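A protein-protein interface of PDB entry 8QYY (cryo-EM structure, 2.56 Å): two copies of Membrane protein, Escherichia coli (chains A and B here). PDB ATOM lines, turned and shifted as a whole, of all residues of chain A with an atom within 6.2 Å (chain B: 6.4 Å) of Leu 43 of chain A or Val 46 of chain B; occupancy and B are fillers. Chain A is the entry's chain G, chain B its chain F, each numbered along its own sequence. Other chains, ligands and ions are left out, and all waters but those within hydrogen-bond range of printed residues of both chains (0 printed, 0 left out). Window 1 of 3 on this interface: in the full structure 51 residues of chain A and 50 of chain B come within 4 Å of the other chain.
N of Met 39 of chain B lies close to SD of Met 39 of chain A (3.7 Å).
OG1 of Thr 47 of chain A sits at hydrogen-bond distance from NE2 of Gln 51 of chain A.
The side-chain hydroxyl of Thr 47 of chain A sits at hydrogen-bond distance from the backbone carbonyl oxygen of Leu 43 of chain A.
O of Leu 43 of chain B lies within hydrogen-bond range of OG1 of Thr 47 of chain B, at 3.0 Å.
The backbone carbonyl oxygen of Val 38 of chain A lies within hydrogen-bond range of the side-chain hydroxyl of Ser 42 of chain A (2.6 Å).
Among the printed residues, merely in contact across the chains: Val 38 of chain A with Met 39 of chain B, Thr 47 of chain A with Val 46 of chain B, Ser 42 of chain A with Leu 43 of chain B, Leu 43 of chain A with Val 46 of chain B, Val 46 of chain A with Ile 50 of chain B, Leu 43 of chain A with Ser 42 of chain B and Leu 43 of chain A with Leu 43 of chain B.
Leu 43 of chain A touches just these residues of chain B: Ser 42, Leu 43 and Val 46.
Of chain A, only Leu 43 and Thr 47 come within 4 Å of Val 46 of chain B.
Of the printed residues of chain B, Val 38 of chain A touches Met 39.
Of the printed residues of chain B, Val 46 of chain A touches Ile 50.
Printed residues of chain A within 4 Å of Ser 42 of chain B: Leu 43.
Printed residues of chain A within 4 Å of Leu 43 of chain B: Ser 42 (3.7 Å) and Leu 43 (3.98 Å).
Ser 45 of chain B touches none of the printed residues of chain A.
Gln 48 of chain A touches none of the printed residues of chain B.
The nearest residue of chain B that does not touch Leu 43 of chain A is Met 39 of chain B (6.0 Å).
Hydrophobic or aromatic side chains of chain A within 4 Å of the printed part of chain B: Val 38, Met 39 and Leu 43.
Of the 12 printed residues of chain B, 5 touch a printed residue of chain A.
Met 39 of chain A touches its own counterpart, Met 39 of chain B.
Ser 42 of chain A touches Leu 43 of chain B, and with the chains exchanged Leu 43 of chain A touches Ser 42 of chain B.
Leu 43 of chain B touches its own counterpart, Leu 43 of chain A.
Thr 47 of chain A touches Val 46 of chain B, but with the chains exchanged Val 46 of chain A does not touch Thr 47 of chain B (4.5 Å).
Positions printed for both chains: 39, 41, 42, 43, 44, 45, 46, 47, 48 and 51.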
ATOM      1  N   VAL A  38      -0.684 -23.887  24.268  1.00  0.00           N
ATOM      2  CA  VAL A  38       0.133 -22.919  23.552  1.00  0.00           C
ATOM      3  C   VAL A  38      -0.175 -21.508  24.033  1.00  0.00           C
ATOM      4  O   VAL A  38       0.730 -20.680  24.179  1.00  0.00           O
ATOM      5  CB  VAL A  38      -0.070 -23.070  22.034  1.00  0.00           C
ATOM      6  CG1 VAL A  38       0.441 -21.849  21.294  1.00  0.00           C
ATOM      7  CG2 VAL A  38       0.621 -24.318  21.551  1.00  0.00           C
ATOM      8  N   MET A  39      -1.449 -21.215  24.312  1.00  0.00           N
ATOM      9  CA  MET A  39      -1.787 -19.933  24.918  1.00  0.00           C
ATOM     10  C   MET A  39      -1.114 -19.768  26.271  1.00  0.00           C
ATOM     11  O   MET A  39      -0.573 -18.702  26.578  1.00  0.00           O
ATOM     12  CB  MET A  39      -3.301 -19.805  25.072  1.00  0.00           C
ATOM     13  CG  MET A  39      -3.743 -18.477  25.649  1.00  0.00           C
ATOM     14  SD  MET A  39      -5.527 -18.353  25.789  1.00  0.00           S
ATOM     15  CE  MET A  39      -5.815 -19.480  27.138  1.00  0.00           C
ATOM     16  N   VAL A  40      -1.144 -20.816  27.094  1.00  0.00           N
ATOM     17  CA  VAL A  40      -0.545 -20.738  28.425  1.00  0.00           C
ATOM     18  C   VAL A  40       0.952 -20.485  28.321  1.00  0.00           C
ATOM     19  O   VAL A  40       1.501 -19.612  29.001  1.00  0.00           O
ATOM     20  CB  VAL A  40      -0.847 -22.023  29.216  1.00  0.00           C
ATOM     21  CG1 VAL A  40       0.070 -22.139  30.420  1.00  0.00           C
ATOM     22  CG2 VAL A  40      -2.298 -22.043  29.639  1.00  0.00           C
ATOM     23  N   ALA A  41       1.629 -21.239  27.453  1.00  0.00           N
ATOM     24  CA  ALA A  41       3.069 -21.073  27.283  1.00  0.00           C
ATOM     25  C   ALA A  41       3.411 -19.694  26.736  1.00  0.00           C
ATOM     26  O   ALA A  41       4.351 -19.048  27.207  1.00  0.00           O
ATOM     27  CB  ALA A  41       3.614 -22.163  26.362  1.00  0.00           C
ATOM     28  N   SER A  42       2.656 -19.222  25.743  1.00  0.00           N
ATOM     29  CA  SER A  42       2.940 -17.923  25.151  1.00  0.00           C
ATOM     30  C   SER A  42       2.730 -16.797  26.153  1.00  0.00           C
ATOM     31  O   SER A  42       3.547 -15.872  26.232  1.00  0.00           O
ATOM     32  CB  SER A  42       2.067 -17.718  23.917  1.00  0.00           C
ATOM     33  OG  SER A  42       2.148 -18.833  23.052  1.00  0.00           O
ATOM     34  N   LEU A  43       1.642 -16.854  26.922  1.00  0.00           N
ATOM     35  CA  LEU A  43       1.388 -15.816  27.914  1.00  0.00           C
ATOM     36  C   LEU A  43       2.420 -15.856  29.030  1.00  0.00           C
ATOM     37  O   LEU A  43       2.860 -14.807  29.509  1.00  0.00           O
ATOM     38  CB  LEU A  43      -0.023 -15.960  28.477  1.00  0.00           C
ATOM     39  CG  LEU A  43      -1.147 -15.573  27.519  1.00  0.00           C
ATOM     40  CD1 LEU A  43      -2.497 -15.733  28.186  1.00  0.00           C
ATOM     41  CD2 LEU A  43      -0.955 -14.155  27.029  1.00  0.00           C
ATOM     42  N   SER A  44       2.821 -17.053  29.460  1.00  0.00           N
ATOM     43  CA  SER A  44       3.859 -17.160  30.475  1.00  0.00           C
ATOM     44  C   SER A  44       5.220 -16.730  29.952  1.00  0.00           C
ATOM     45  O   SER A  44       6.090 -16.368  30.752  1.00  0.00           O
ATOM     46  CB  SER A  44       3.928 -18.592  31.002  1.00  0.00           C
ATOM     47  OG  SER A  44       2.661 -19.018  31.464  1.00  0.00           O
ATOM     48  N   SER A  45       5.428 -16.768  28.637  1.00  0.00           N
ATOM     49  CA  SER A  45       6.706 -16.351  28.078  1.00  0.00           C
ATOM     50  C   SER A  45       6.772 -14.841  27.878  1.00  0.00           C
ATOM     51  O   SER A  45       7.794 -14.218  28.177  1.00  0.00           O
ATOM     52  CB  SER A  45       6.961 -17.080  26.760  1.00  0.00           C
ATOM     53  OG  SER A  45       6.859 -18.481  26.934  1.00  0.00           O
ATOM     54  N   VAL A  46       5.698 -14.234  27.369  1.00  0.00           N
ATOM     55  CA  VAL A  46       5.739 -12.797  27.101  1.00  0.00           C
ATOM     56  C   VAL A  46       5.840 -12.009  28.400  1.00  0.00           C
ATOM     57  O   VAL A  46       6.482 -10.953  28.453  1.00  0.00           O
ATOM     58  CB  VAL A  46       4.526 -12.350  26.267  1.00  0.00           C
ATOM     59  CG1 VAL A  46       4.655 -12.829  24.839  1.00  0.00           C
ATOM     60  CG2 VAL A  46       3.236 -12.830  26.885  1.00  0.00           C
ATOM     61  N   THR A  47       5.211 -12.498  29.466  1.00  0.00           N
ATOM     62  CA  THR A  47       5.156 -11.774  30.728  1.00  0.00           C
ATOM     63  C   THR A  47       6.165 -12.281  31.748  1.00  0.00           C
ATOM     64  O   THR A  47       6.074 -11.914  32.924  1.00  0.00           O
ATOM     65  CB  THR A  47       3.749 -11.839  31.321  1.00  0.00           C
ATOM     66  OG1 THR A  47       3.541 -13.124  31.916  1.00  0.00           O
ATOM     67  CG2 THR A  47       2.703 -11.608  30.250  1.00  0.00           C
ATOM     68  N   GLN A  48       7.129 -13.107  31.335  1.00  0.00           N
ATOM     69  CA  GLN A  48       8.049 -13.676  32.316  1.00  0.00           C
ATOM     70  C   GLN A  48       8.938 -12.605  32.932  1.00  0.00           C
ATOM     71  O   GLN A  48       9.298 -12.699  34.108  1.00  0.00           O
ATOM     72  CB  GLN A  48       8.895 -14.788  31.697  1.00  0.00           C
ATOM     73  CG  GLN A  48       9.852 -14.359  30.610  1.00  0.00           C
ATOM     74  CD  GLN A  48      10.602 -15.537  30.027  1.00  0.00           C
ATOM     75  OE1 GLN A  48      10.437 -16.671  30.474  1.00  0.00           O
ATOM     76  NE2 GLN A  48      11.435 -15.276  29.031  1.00  0.00           N
ATOM     77  N   GLN A  51       6.580 -11.066  35.321  1.00  0.00           N
ATOM     78  CA  GLN A  51       6.418 -11.970  36.456  1.00  0.00           C
ATOM     79  C   GLN A  51       7.619 -11.901  37.390  1.00  0.00           C
ATOM     80  O   GLN A  51       7.465 -11.877  38.614  1.00  0.00           O
ATOM     81  CB  GLN A  51       6.205 -13.404  35.974  1.00  0.00           C
ATOM     82  CG  GLN A  51       4.898 -13.646  35.248  1.00  0.00           C
ATOM     83  CD  GLN A  51       4.758 -15.079  34.781  1.00  0.00           C
ATOM     84  OE1 GLN A  51       5.670 -15.886  34.943  1.00  0.00           O
ATOM     85  NE2 GLN A  51       3.609 -15.403  34.198  1.00  0.00           N
ATOM     86  N   MET B  39      -6.792 -17.641  22.360  1.00  0.00           N
ATOM     87  CA  MET B  39      -5.334 -17.645  22.323  1.00  0.00           C
ATOM     88  C   MET B  39      -4.798 -16.435  21.579  1.00  0.00           C
ATOM     89  O   MET B  39      -3.986 -15.669  22.116  1.00  0.00           O
ATOM     90  CB  MET B  39      -4.832 -18.922  21.656  1.00  0.00           C
ATOM     91  CG  MET B  39      -3.323 -19.030  21.618  1.00  0.00           C
ATOM     92  SD  MET B  39      -2.759 -20.551  20.846  1.00  0.00           S
ATOM     93  CE  MET B  39      -3.154 -20.228  19.135  1.00  0.00           C
ATOM     94  N   ALA B  41      -6.350 -13.663  20.568  1.00  0.00           N
ATOM     95  CA  ALA B  41      -6.802 -12.399  21.132  1.00  0.00           C
ATOM     96  C   ALA B  41      -6.059 -12.061  22.418  1.00  0.00           C
ATOM     97  O   ALA B  41      -5.653 -10.913  22.615  1.00  0.00           O
ATOM     98  CB  ALA B  41      -8.308 -12.445  21.380  1.00  0.00           C
ATOM     99  N   SER B  42      -5.862 -13.042  23.301  1.00  0.00           N
ATOM    100  CA  SER B  42      -5.158 -12.794  24.550  1.00  0.00           C
ATOM    101  C   SER B  42      -3.694 -12.469  24.307  1.00  0.00           C
ATOM    102  O   SER B  42      -3.143 -11.569  24.948  1.00  0.00           O
ATOM    103  CB  SER B  42      -5.293 -14.004  25.470  1.00  0.00           C
ATOM    104  OG  SER B  42      -6.565 -14.030  26.090  1.00  0.00           O
ATOM    105  N   LEU B  43      -3.046 -13.184  23.385  1.00  0.00           N
ATOM    106  CA  LEU B  43      -1.654 -12.881  23.079  1.00  0.00           C
ATOM    107  C   LEU B  43      -1.516 -11.471  22.522  1.00  0.00           C
ATOM    108  O   LEU B  43      -0.656 -10.695  22.961  1.00  0.00           O
ATOM    109  CB  LEU B  43      -1.098 -13.910  22.100  1.00  0.00           C
ATOM    110  CG  LEU B  43       0.422 -14.057  22.107  1.00  0.00           C
ATOM    111  CD1 LEU B  43       0.927 -14.264  23.525  1.00  0.00           C
ATOM    112  CD2 LEU B  43       0.848 -15.200  21.208  1.00  0.00           C
ATOM    113  N   SER B  44      -2.376 -11.113  21.565  1.00  0.00           N
ATOM    114  CA  SER B  44      -2.339  -9.773  20.997  1.00  0.00           C
ATOM    115  C   SER B  44      -2.599  -8.716  22.058  1.00  0.00           C
ATOM    116  O   SER B  44      -1.893  -7.706  22.122  1.00  0.00           O
ATOM    117  CB  SER B  44      -3.360  -9.662  19.865  1.00  0.00           C
ATOM    118  OG  SER B  44      -3.362  -8.365  19.302  1.00  0.00           O
ATOM    119  N   SER B  45      -3.597  -8.939  22.918  1.00  0.00           N
ATOM    120  CA  SER B  45      -3.936  -7.960  23.942  1.00  0.00           C
ATOM    121  C   SER B  45      -2.803  -7.773  24.941  1.00  0.00           C
ATOM    122  O   SER B  45      -2.463  -6.641  25.294  1.00  0.00           O
ATOM    123  CB  SER B  45      -5.217  -8.386  24.657  1.00  0.00           C
ATOM    124  OG  SER B  45      -5.502  -7.534  25.748  1.00  0.00           O
ATOM    125  N   VAL B  46      -2.207  -8.868  25.414  1.00  0.00           N
ATOM    126  CA  VAL B  46      -1.135  -8.754  26.394  1.00  0.00           C
ATOM    127  C   VAL B  46       0.079  -8.069  25.781  1.00  0.00           C
ATOM    128  O   VAL B  46       0.707  -7.208  26.412  1.00  0.00           O
ATOM    129  CB  VAL B  46      -0.782 -10.138  26.966  1.00  0.00           C
ATOM    130  CG1 VAL B  46       0.472 -10.056  27.809  1.00  0.00           C
ATOM    131  CG2 VAL B  46      -1.937 -10.667  27.794  1.00  0.00           C
ATOM    132  N   THR B  47       0.425  -8.427  24.543  1.00  0.00           N
ATOM    133  CA  THR B  47       1.530  -7.753  23.875  1.00  0.00           C
ATOM    134  C   THR B  47       1.237  -6.267  23.699  1.00  0.00           C
ATOM    135  O   THR B  47       2.138  -5.430  23.832  1.00  0.00           O
ATOM    136  CB  THR B  47       1.805  -8.418  22.529  1.00  0.00           C
ATOM    137  OG1 THR B  47       2.149  -9.792  22.744  1.00  0.00           O
ATOM    138  CG2 THR B  47       2.950  -7.726  21.811  1.00  0.00           C
ATOM    139  N   GLN B  48      -0.019  -5.919  23.409  1.00  0.00           N
ATOM    140  CA  GLN B  48      -0.373  -4.515  23.245  1.00  0.00           C
ATOM    141  C   GLN B  48      -0.268  -3.754  24.561  1.00  0.00           C
ATOM    142  O   GLN B  48       0.207  -2.618  24.577  1.00  0.00           O
ATOM    143  CB  GLN B  48      -1.775  -4.385  22.653  1.00  0.00           C
ATOM    144  CG  GLN B  48      -1.857  -4.759  21.183  1.00  0.00           C
ATOM    145  CD  GLN B  48      -3.193  -4.409  20.565  1.00  0.00           C
ATOM    146  OE1 GLN B  48      -3.680  -3.290  20.708  1.00  0.00           O
ATOM    147  NE2 GLN B  48      -3.796  -5.369  19.876  1.00  0.00           N
ATOM    148  N   ARG B  49      -0.705  -4.354  25.673  1.00  0.00           N
ATOM    149  CA  ARG B  49      -0.479  -3.724  26.976  1.00  0.00           C
ATOM    150  C   ARG B  49       1.004  -3.518  27.252  1.00  0.00           C
ATOM    151  O   ARG B  49       1.413  -2.454  27.732  1.00  0.00           O
ATOM    152  CB  ARG B  49      -1.110  -4.531  28.114  1.00  0.00           C
ATOM    153  CG  ARG B  49      -2.577  -4.264  28.402  1.00  0.00           C
ATOM    154  CD  ARG B  49      -3.531  -4.848  27.417  1.00  0.00           C
ATOM    155  NE  ARG B  49      -4.910  -4.601  27.815  1.00  0.00           N
ATOM    156  CZ  ARG B  49      -5.613  -5.395  28.607  1.00  0.00           C
ATOM    157  NH1 ARG B  49      -5.096  -6.507  29.103  1.00  0.00           N
ATOM    158  NH2 ARG B  49      -6.866  -5.067  28.907  1.00  0.00           N
ATOM    159  N   ILE B  50       1.827  -4.530  26.975  1.00  0.00           N
ATOM    160  CA  ILE B  50       3.254  -4.411  27.270  1.00  0.00           C
ATOM    161  C   ILE B  50       3.881  -3.291  26.448  1.00  0.00           C
ATOM    162  O   ILE B  50       4.604  -2.434  26.978  1.00  0.00           O
ATOM    163  CB  ILE B  50       3.964  -5.756  27.036  1.00  0.00           C
ATOM    164  CG1 ILE B  50       3.423  -6.817  27.993  1.00  0.00           C
ATOM    165  CG2 ILE B  50       5.463  -5.605  27.211  1.00  0.00           C
ATOM    166  CD1 ILE B  50       3.874  -8.214  27.664  1.00  0.00           C
ATOM    167  N   GLN B  51       3.600  -3.266  25.142  1.00  0.00           N
ATOM    168  CA  GLN B  51       4.189  -2.228  24.305  1.00  0.00           C
ATOM    169  C   GLN B  51       3.604  -0.858  24.622  1.00  0.00           C
ATOM    170  O   GLN B  51       4.316   0.145  24.535  1.00  0.00           O
ATOM    171  CB  GLN B  51       4.018  -2.561  22.821  1.00  0.00           C
ATOM    172  CG  GLN B  51       2.589  -2.572  22.318  1.00  0.00           C
ATOM    173  CD  GLN B  51       2.496  -2.966  20.856  1.00  0.00           C
ATOM    174  OE1 GLN B  51       3.510  -3.189  20.195  1.00  0.00           O
ATOM    175  NE2 GLN B  51       1.274  -3.044  20.341  1.00  0.00           N
